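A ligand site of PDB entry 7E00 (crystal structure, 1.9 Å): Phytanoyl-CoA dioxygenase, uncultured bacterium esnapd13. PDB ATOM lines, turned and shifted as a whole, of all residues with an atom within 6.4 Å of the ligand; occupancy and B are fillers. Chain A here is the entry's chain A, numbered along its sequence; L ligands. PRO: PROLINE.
The indole nitrogen (NE1) of Trp 122 sits at hydrogen-bond distance from an oxygen (O) of the ligand.
The guanidinium group (NH1) of Arg 248 lies within salt-bridge range of an oxygen (OXT) of the ligand, at 2.7 Å.
The side-chain amide nitrogen of Gln 99 sits at hydrogen-bond distance from an oxygen (O) of the ligand (3.2 Å).
The backbone carbonyl oxygen (O) of Thr 174 lies within hydrogen-bond range of a nitrogen (N) of the ligand (3.1 Å).
OD2 of Asp 126 lies within salt-bridge range of NH2 of Arg 248, 2.7 Å away.
The backbone carbonyl oxygen (O) of Leu 252 lies within hydrogen-bond range of the side-chain amide nitrogen (NE2) of Gln 99, 2.9 Å away.
The guanidinium group (NH1) of Arg 248 sits at hydrogen-bond distance from the side-chain hydroxyl (OG1) of Thr 174, 3.1 Å away.
The backbone carbonyl oxygen of His 116 sits at hydrogen-bond distance from the backbone NH of His 216.
OD1 of Asp 118 lies within hydrogen-bond range of NE2 of His 116, at 3.3 Å.
The side-chain hydroxyl (OG1) of Thr 174 is in hydrogen-bond range of the backbone carbonyl oxygen (O) of Trp 171.
OE1 of Gln 99 lies within hydrogen-bond range of NZ of Lys 101, 2.8 Å away.
Residues that only touch the ligand: Asp 118, Phe 121, His 116 and Lys 101.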
ATOM      1  N   HIS A  65     -22.201   3.354 -11.242  1.00  0.00           N
ATOM      2  CA  HIS A  65     -22.018   2.863  -9.915  1.00  0.00           C
ATOM      3  C   HIS A  65     -20.535   2.910  -9.478  1.00  0.00           C
ATOM      4  O   HIS A  65     -19.651   2.642 -10.212  1.00  0.00           O
ATOM      5  CB  HIS A  65     -22.615   1.450  -9.741  1.00  0.00           C
ATOM      6  CG  HIS A  65     -24.083   1.393 -10.037  1.00  0.00           C
ATOM      7  ND1 HIS A  65     -24.592   1.574 -11.317  1.00  0.00           N
ATOM      8  CD2 HIS A  65     -25.158   1.256  -9.225  1.00  0.00           C
ATOM      9  CE1 HIS A  65     -25.909   1.610 -11.259  1.00  0.00           C
ATOM     10  NE2 HIS A  65     -26.285   1.383 -10.010  1.00  0.00           N
ATOM     11  N   HIS A  98     -21.347   2.418   1.532  1.00  0.00           N
ATOM     12  CA  HIS A  98     -21.750   1.121   1.091  1.00  0.00           C
ATOM     13  C   HIS A  98     -21.908   1.059  -0.459  1.00  0.00           C
ATOM     14  O   HIS A  98     -21.392   0.146  -1.142  1.00  0.00           O
ATOM     15  CB  HIS A  98     -23.057   0.672   1.736  1.00  0.00           C
ATOM     16  CG  HIS A  98     -23.597  -0.604   1.155  1.00  0.00           C
ATOM     17  ND1 HIS A  98     -22.869  -1.780   1.154  1.00  0.00           N
ATOM     18  CD2 HIS A  98     -24.747  -0.885   0.498  1.00  0.00           C
ATOM     19  CE1 HIS A  98     -23.546  -2.719   0.520  1.00  0.00           C
ATOM     20  NE2 HIS A  98     -24.685  -2.202   0.107  1.00  0.00           N
ATOM     21  N   GLN A  99     -22.517   2.104  -0.992  1.00  0.00           N
ATOM     22  CA  GLN A  99     -22.821   2.205  -2.427  1.00  0.00           C
ATOM     23  C   GLN A  99     -22.864   3.668  -2.827  1.00  0.00           C
ATOM     24  O   GLN A  99     -23.225   4.535  -2.039  1.00  0.00           O
ATOM     25  CB  GLN A  99     -24.169   1.512  -2.661  1.00  0.00           C
ATOM     26  CG  GLN A  99     -24.689   1.645  -4.080  1.00  0.00           C
ATOM     27  CD  GLN A  99     -25.865   0.721  -4.297  1.00  0.00           C
ATOM     28  OE1 GLN A  99     -26.972   1.143  -4.157  1.00  0.00           O
ATOM     29  NE2 GLN A  99     -25.591  -0.545  -4.491  1.00  0.00           N
ATOM     30  N   LYS A 101     -23.973   5.914  -6.393  1.00  0.00           N
ATOM     31  CA  LYS A 101     -24.495   5.810  -7.773  1.00  0.00           C
ATOM     32  C   LYS A 101     -24.999   7.130  -8.264  1.00  0.00           C
ATOM     33  O   LYS A 101     -25.353   8.017  -7.486  1.00  0.00           O
ATOM     34  CB  LYS A 101     -25.554   4.709  -7.873  1.00  0.00           C
ATOM     35  CG  LYS A 101     -26.797   4.918  -7.013  1.00  0.00           C
ATOM     36  CD  LYS A 101     -27.701   3.665  -6.902  1.00  0.00           C
ATOM     37  CE  LYS A 101     -28.806   3.842  -5.859  1.00  0.00           C
ATOM     38  NZ  LYS A 101     -28.316   3.531  -4.482  1.00  0.00           N
ATOM     39  N   TRP A 113     -38.121   3.653 -12.022  1.00  0.00           N
ATOM     40  CA  TRP A 113     -37.700   2.776 -10.911  1.00  0.00           C
ATOM     41  C   TRP A 113     -38.942   2.255 -10.177  1.00  0.00           C
ATOM     42  O   TRP A 113     -39.639   3.048  -9.548  1.00  0.00           O
ATOM     43  CB  TRP A 113     -36.800   3.553  -9.896  1.00  0.00           C
ATOM     44  CG  TRP A 113     -35.404   3.770 -10.409  1.00  0.00           C
ATOM     45  CD1 TRP A 113     -34.926   4.893 -11.033  1.00  0.00           C
ATOM     46  CD2 TRP A 113     -34.299   2.820 -10.382  1.00  0.00           C
ATOM     47  NE1 TRP A 113     -33.609   4.706 -11.379  1.00  0.00           N
ATOM     48  CE2 TRP A 113     -33.190   3.452 -10.982  1.00  0.00           C
ATOM     49  CE3 TRP A 113     -34.169   1.500  -9.914  1.00  0.00           C
ATOM     50  CZ2 TRP A 113     -31.933   2.787 -11.160  1.00  0.00           C
ATOM     51  CZ3 TRP A 113     -32.896   0.842 -10.044  1.00  0.00           C
ATOM     52  CH2 TRP A 113     -31.814   1.485 -10.662  1.00  0.00           C
ATOM     53  N   HIS A 116     -39.507  -0.104  -4.142  1.00  0.00           N
ATOM     54  CA  HIS A 116     -38.534  -0.947  -3.428  1.00  0.00           C
ATOM     55  C   HIS A 116     -38.017  -0.318  -2.151  1.00  0.00           C
ATOM     56  O   HIS A 116     -38.186   0.835  -1.891  1.00  0.00           O
ATOM     57  CB  HIS A 116     -37.386  -1.381  -4.297  1.00  0.00           C
ATOM     58  CG  HIS A 116     -36.490  -0.244  -4.704  1.00  0.00           C
ATOM     59  ND1 HIS A 116     -36.907   0.792  -5.505  1.00  0.00           N
ATOM     60  CD2 HIS A 116     -35.206   0.043  -4.372  1.00  0.00           C
ATOM     61  CE1 HIS A 116     -35.926   1.670  -5.656  1.00  0.00           C
ATOM     62  NE2 HIS A 116     -34.882   1.238  -4.981  1.00  0.00           N
ATOM     63  N   GLN A 117     -37.508  -1.165  -1.279  1.00  0.00           N
ATOM     64  CA  GLN A 117     -36.714  -0.757  -0.119  1.00  0.00           C
ATOM     65  C   GLN A 117     -35.310  -1.161  -0.456  1.00  0.00           C
ATOM     66  O   GLN A 117     -35.016  -2.369  -0.731  1.00  0.00           O
ATOM     67  CB  GLN A 117     -37.183  -1.462   1.134  1.00  0.00           C
ATOM     68  CG  GLN A 117     -38.552  -1.015   1.661  1.00  0.00           C
ATOM     69  CD  GLN A 117     -39.186  -2.045   2.645  1.00  0.00           C
ATOM     70  OE1 GLN A 117     -39.329  -3.214   2.324  1.00  0.00           O
ATOM     71  NE2 GLN A 117     -39.588  -1.580   3.794  1.00  0.00           N
ATOM     72  N   ASP A 118     -34.419  -0.186  -0.400  1.00  0.00           N
ATOM     73  CA  ASP A 118     -32.962  -0.476  -0.601  1.00  0.00           C
ATOM     74  C   ASP A 118     -32.439  -1.609   0.322  1.00  0.00           C
ATOM     75  O   ASP A 118     -31.668  -2.444  -0.111  1.00  0.00           O
ATOM     76  CB  ASP A 118     -32.102   0.830  -0.312  1.00  0.00           C
ATOM     77  CG  ASP A 118     -32.287   1.938  -1.399  1.00  0.00           C
ATOM     78  OD1 ASP A 118     -32.665   1.556  -2.535  1.00  0.00           O
ATOM     79  OD2 ASP A 118     -31.984   3.151  -1.122  1.00  0.00           O
ATOM     80  N   PHE A 121     -32.564  -5.204  -0.814  1.00  0.00           N
ATOM     81  CA  PHE A 121     -31.450  -5.524  -1.689  1.00  0.00           C
ATOM     82  C   PHE A 121     -30.145  -5.784  -0.921  1.00  0.00           C
ATOM     83  O   PHE A 121     -29.414  -6.766  -1.178  1.00  0.00           O
ATOM     84  CB  PHE A 121     -31.115  -4.431  -2.703  1.00  0.00           C
ATOM     85  CG  PHE A 121     -32.163  -4.263  -3.784  1.00  0.00           C
ATOM     86  CD1 PHE A 121     -33.440  -3.754  -3.480  1.00  0.00           C
ATOM     87  CD2 PHE A 121     -31.854  -4.613  -5.106  1.00  0.00           C
ATOM     88  CE1 PHE A 121     -34.402  -3.638  -4.482  1.00  0.00           C
ATOM     89  CE2 PHE A 121     -32.818  -4.463  -6.103  1.00  0.00           C
ATOM     90  CZ  PHE A 121     -34.088  -3.990  -5.790  1.00  0.00           C
ATOM     91  N   TRP A 122     -29.821  -4.849  -0.041  1.00  0.00           N
ATOM     92  CA  TRP A 122     -28.483  -4.880   0.586  1.00  0.00           C
ATOM     93  C   TRP A 122     -28.424  -6.027   1.603  1.00  0.00           C
ATOM     94  O   TRP A 122     -27.401  -6.598   1.782  1.00  0.00           O
ATOM     95  CB  TRP A 122     -28.188  -3.523   1.294  1.00  0.00           C
ATOM     96  CG  TRP A 122     -28.163  -2.362   0.296  1.00  0.00           C
ATOM     97  CD1 TRP A 122     -27.819  -2.420  -1.013  1.00  0.00           C
ATOM     98  CD2 TRP A 122     -28.519  -1.009   0.551  1.00  0.00           C
ATOM     99  NE1 TRP A 122     -27.981  -1.191  -1.607  1.00  0.00           N
ATOM    100  CE2 TRP A 122     -28.389  -0.306  -0.657  1.00  0.00           C
ATOM    101  CE3 TRP A 122     -28.866  -0.331   1.696  1.00  0.00           C
ATOM    102  CZ2 TRP A 122     -28.538   1.060  -0.744  1.00  0.00           C
ATOM    103  CZ3 TRP A 122     -29.093   1.044   1.598  1.00  0.00           C
ATOM    104  CH2 TRP A 122     -28.959   1.716   0.362  1.00  0.00           C
ATOM    105  N   GLU A 125     -28.519  -9.275  -1.074  1.00  0.00           N
ATOM    106  CA  GLU A 125     -27.429  -9.378  -2.010  1.00  0.00           C
ATOM    107  C   GLU A 125     -26.075  -9.222  -1.332  1.00  0.00           C
ATOM    108  O   GLU A 125     -25.081  -9.731  -1.859  1.00  0.00           O
ATOM    109  CB  GLU A 125     -27.521  -8.342  -3.131  1.00  0.00           C
ATOM    110  CG  GLU A 125     -28.812  -8.346  -3.923  1.00  0.00           C
ATOM    111  CD  GLU A 125     -28.867  -9.510  -4.901  1.00  0.00           C
ATOM    112  OE1 GLU A 125     -28.098  -9.492  -5.882  1.00  0.00           O
ATOM    113  OE2 GLU A 125     -29.691 -10.437  -4.663  1.00  0.00           O
ATOM    114  N   ASP A 126     -26.020  -8.436  -0.266  1.00  0.00           N
ATOM    115  CA  ASP A 126     -24.696  -7.984   0.219  1.00  0.00           C
ATOM    116  C   ASP A 126     -24.389  -8.378   1.617  1.00  0.00           C
ATOM    117  O   ASP A 126     -23.256  -8.194   2.008  1.00  0.00           O
ATOM    118  CB  ASP A 126     -24.533  -6.473   0.082  1.00  0.00           C
ATOM    119  CG  ASP A 126     -24.796  -5.979  -1.303  1.00  0.00           C
ATOM    120  OD1 ASP A 126     -24.337  -6.623  -2.300  1.00  0.00           O
ATOM    121  OD2 ASP A 126     -25.412  -4.892  -1.377  1.00  0.00           O
ATOM    122  N   TRP A 171     -27.357 -10.745 -10.181  1.00  0.00           N
ATOM    123  CA  TRP A 171     -27.422  -9.319  -9.731  1.00  0.00           C
ATOM    124  C   TRP A 171     -27.637  -8.286 -10.835  1.00  0.00           C
ATOM    125  O   TRP A 171     -27.973  -7.149 -10.478  1.00  0.00           O
ATOM    126  CB  TRP A 171     -26.252  -8.891  -8.842  1.00  0.00           C
ATOM    127  CG  TRP A 171     -24.885  -9.133  -9.372  1.00  0.00           C
ATOM    128  CD1 TRP A 171     -24.048 -10.181  -9.044  1.00  0.00           C
ATOM    129  CD2 TRP A 171     -24.171  -8.316 -10.289  1.00  0.00           C
ATOM    130  NE1 TRP A 171     -22.853 -10.049  -9.717  1.00  0.00           N
ATOM    131  CE2 TRP A 171     -22.898  -8.930 -10.499  1.00  0.00           C
ATOM    132  CE3 TRP A 171     -24.458  -7.113 -10.969  1.00  0.00           C
ATOM    133  CZ2 TRP A 171     -21.944  -8.399 -11.351  1.00  0.00           C
ATOM    134  CZ3 TRP A 171     -23.523  -6.605 -11.829  1.00  0.00           C
ATOM    135  CH2 TRP A 171     -22.267  -7.246 -12.012  1.00  0.00           C
ATOM    136  N   THR A 174     -30.653  -6.065 -10.468  1.00  0.00           N
ATOM    137  CA  THR A 174     -30.717  -5.174  -9.260  1.00  0.00           C
ATOM    138  C   THR A 174     -30.855  -3.643  -9.602  1.00  0.00           C
ATOM    139  O   THR A 174     -31.489  -2.857  -8.893  1.00  0.00           O
ATOM    140  CB  THR A 174     -29.552  -5.463  -8.228  1.00  0.00           C
ATOM    141  OG1 THR A 174     -28.247  -5.296  -8.807  1.00  0.00           O
ATOM    142  CG2 THR A 174     -29.686  -6.913  -7.637  1.00  0.00           C
ATOM    143  N   LEU A 175     -30.333  -3.245 -10.753  1.00  0.00           N
ATOM    144  CA  LEU A 175     -30.455  -1.851 -11.193  1.00  0.00           C
ATOM    145  C   LEU A 175     -31.091  -1.678 -12.611  1.00  0.00           C
ATOM    146  O   LEU A 175     -30.755  -0.723 -13.303  1.00  0.00           O
ATOM    147  CB  LEU A 175     -29.096  -1.149 -11.074  1.00  0.00           C
ATOM    148  CG  LEU A 175     -27.884  -1.990 -11.497  1.00  0.00           C
ATOM    149  CD1 LEU A 175     -26.839  -1.206 -12.233  1.00  0.00           C
ATOM    150  CD2 LEU A 175     -27.230  -2.682 -10.311  1.00  0.00           C
ATOM    151  N   LEU A 179     -36.952  -4.459 -11.474  1.00  0.00           N
ATOM    152  CA  LEU A 179     -36.146  -4.749 -10.262  1.00  0.00           C
ATOM    153  C   LEU A 179     -36.299  -6.161  -9.706  1.00  0.00           C
ATOM    154  O   LEU A 179     -37.418  -6.671  -9.620  1.00  0.00           O
ATOM    155  CB  LEU A 179     -36.594  -3.823  -9.141  1.00  0.00           C
ATOM    156  CG  LEU A 179     -36.374  -2.337  -9.284  1.00  0.00           C
ATOM    157  CD1 LEU A 179     -37.065  -1.651  -8.113  1.00  0.00           C
ATOM    158  CD2 LEU A 179     -34.881  -2.020  -9.332  1.00  0.00           C
ATOM    159  N   HIS A 216     -39.620   3.436  -1.850  1.00  0.00           N
ATOM    160  CA  HIS A 216     -39.625   4.548  -2.745  1.00  0.00           C
ATOM    161  C   HIS A 216     -39.650   4.074  -4.161  1.00  0.00           C
ATOM    162  O   HIS A 216     -39.370   2.896  -4.450  1.00  0.00           O
ATOM    163  CB  HIS A 216     -38.400   5.496  -2.462  1.00  0.00           C
ATOM    164  CG  HIS A 216     -37.077   4.890  -2.758  1.00  0.00           C
ATOM    165  ND1 HIS A 216     -36.454   4.037  -1.884  1.00  0.00           N
ATOM    166  CD2 HIS A 216     -36.221   5.038  -3.805  1.00  0.00           C
ATOM    167  CE1 HIS A 216     -35.278   3.662  -2.372  1.00  0.00           C
ATOM    168  NE2 HIS A 216     -35.119   4.257  -3.541  1.00  0.00           N
ATOM    169  N   ARG A 248     -21.643  -9.403  -4.900  1.00  0.00           N
ATOM    170  CA  ARG A 248     -21.557  -8.325  -5.903  1.00  0.00           C
ATOM    171  C   ARG A 248     -20.197  -7.754  -5.944  1.00  0.00           C
ATOM    172  O   ARG A 248     -19.432  -7.912  -5.021  1.00  0.00           O
ATOM    173  CB  ARG A 248     -22.606  -7.294  -5.621  1.00  0.00           C
ATOM    174  CG  ARG A 248     -23.978  -7.903  -5.655  1.00  0.00           C
ATOM    175  CD  ARG A 248     -25.027  -6.901  -6.039  1.00  0.00           C
ATOM    176  NE  ARG A 248     -25.253  -5.947  -4.946  1.00  0.00           N
ATOM    177  CZ  ARG A 248     -26.155  -4.977  -4.955  1.00  0.00           C
ATOM    178  NH1 ARG A 248     -26.892  -4.738  -6.046  1.00  0.00           N
ATOM    179  NH2 ARG A 248     -26.322  -4.218  -3.860  1.00  0.00           N
ATOM    180  N   LEU A 252     -20.519  -2.012  -6.549  1.00  0.00           N
ATOM    181  CA  LEU A 252     -21.875  -2.019  -6.017  1.00  0.00           C
ATOM    182  C   LEU A 252     -22.028  -2.170  -4.479  1.00  0.00           C
ATOM    183  O   LEU A 252     -23.043  -1.773  -3.907  1.00  0.00           O
ATOM    184  CB  LEU A 252     -22.649  -3.204  -6.637  1.00  0.00           C
ATOM    185  CG  LEU A 252     -23.045  -3.064  -8.097  1.00  0.00           C
ATOM    186  CD1 LEU A 252     -23.825  -4.306  -8.635  1.00  0.00           C
ATOM    187  CD2 LEU A 252     -23.898  -1.837  -8.275  1.00  0.00           C
HETATM  188  N   PRO L   1     -30.654  -0.630  -6.958  1.00  0.00           N
HETATM  189  CA  PRO L   1     -29.571  -0.556  -5.978  1.00  0.00           C
HETATM  190  C   PRO L   1     -28.967  -1.932  -5.599  1.00  0.00           C
HETATM  191  O   PRO L   1     -28.390  -2.108  -4.569  1.00  0.00           O
HETATM  192  CB  PRO L   1     -30.245   0.119  -4.762  1.00  0.00           C
HETATM  193  CG  PRO L   1     -31.659  -0.376  -4.844  1.00  0.00           C
HETATM  194  CD  PRO L   1     -31.985  -0.497  -6.322  1.00  0.00           C
HETATM  195  OXT PRO L   1     -28.965  -2.960  -6.286  1.00  0.00           O
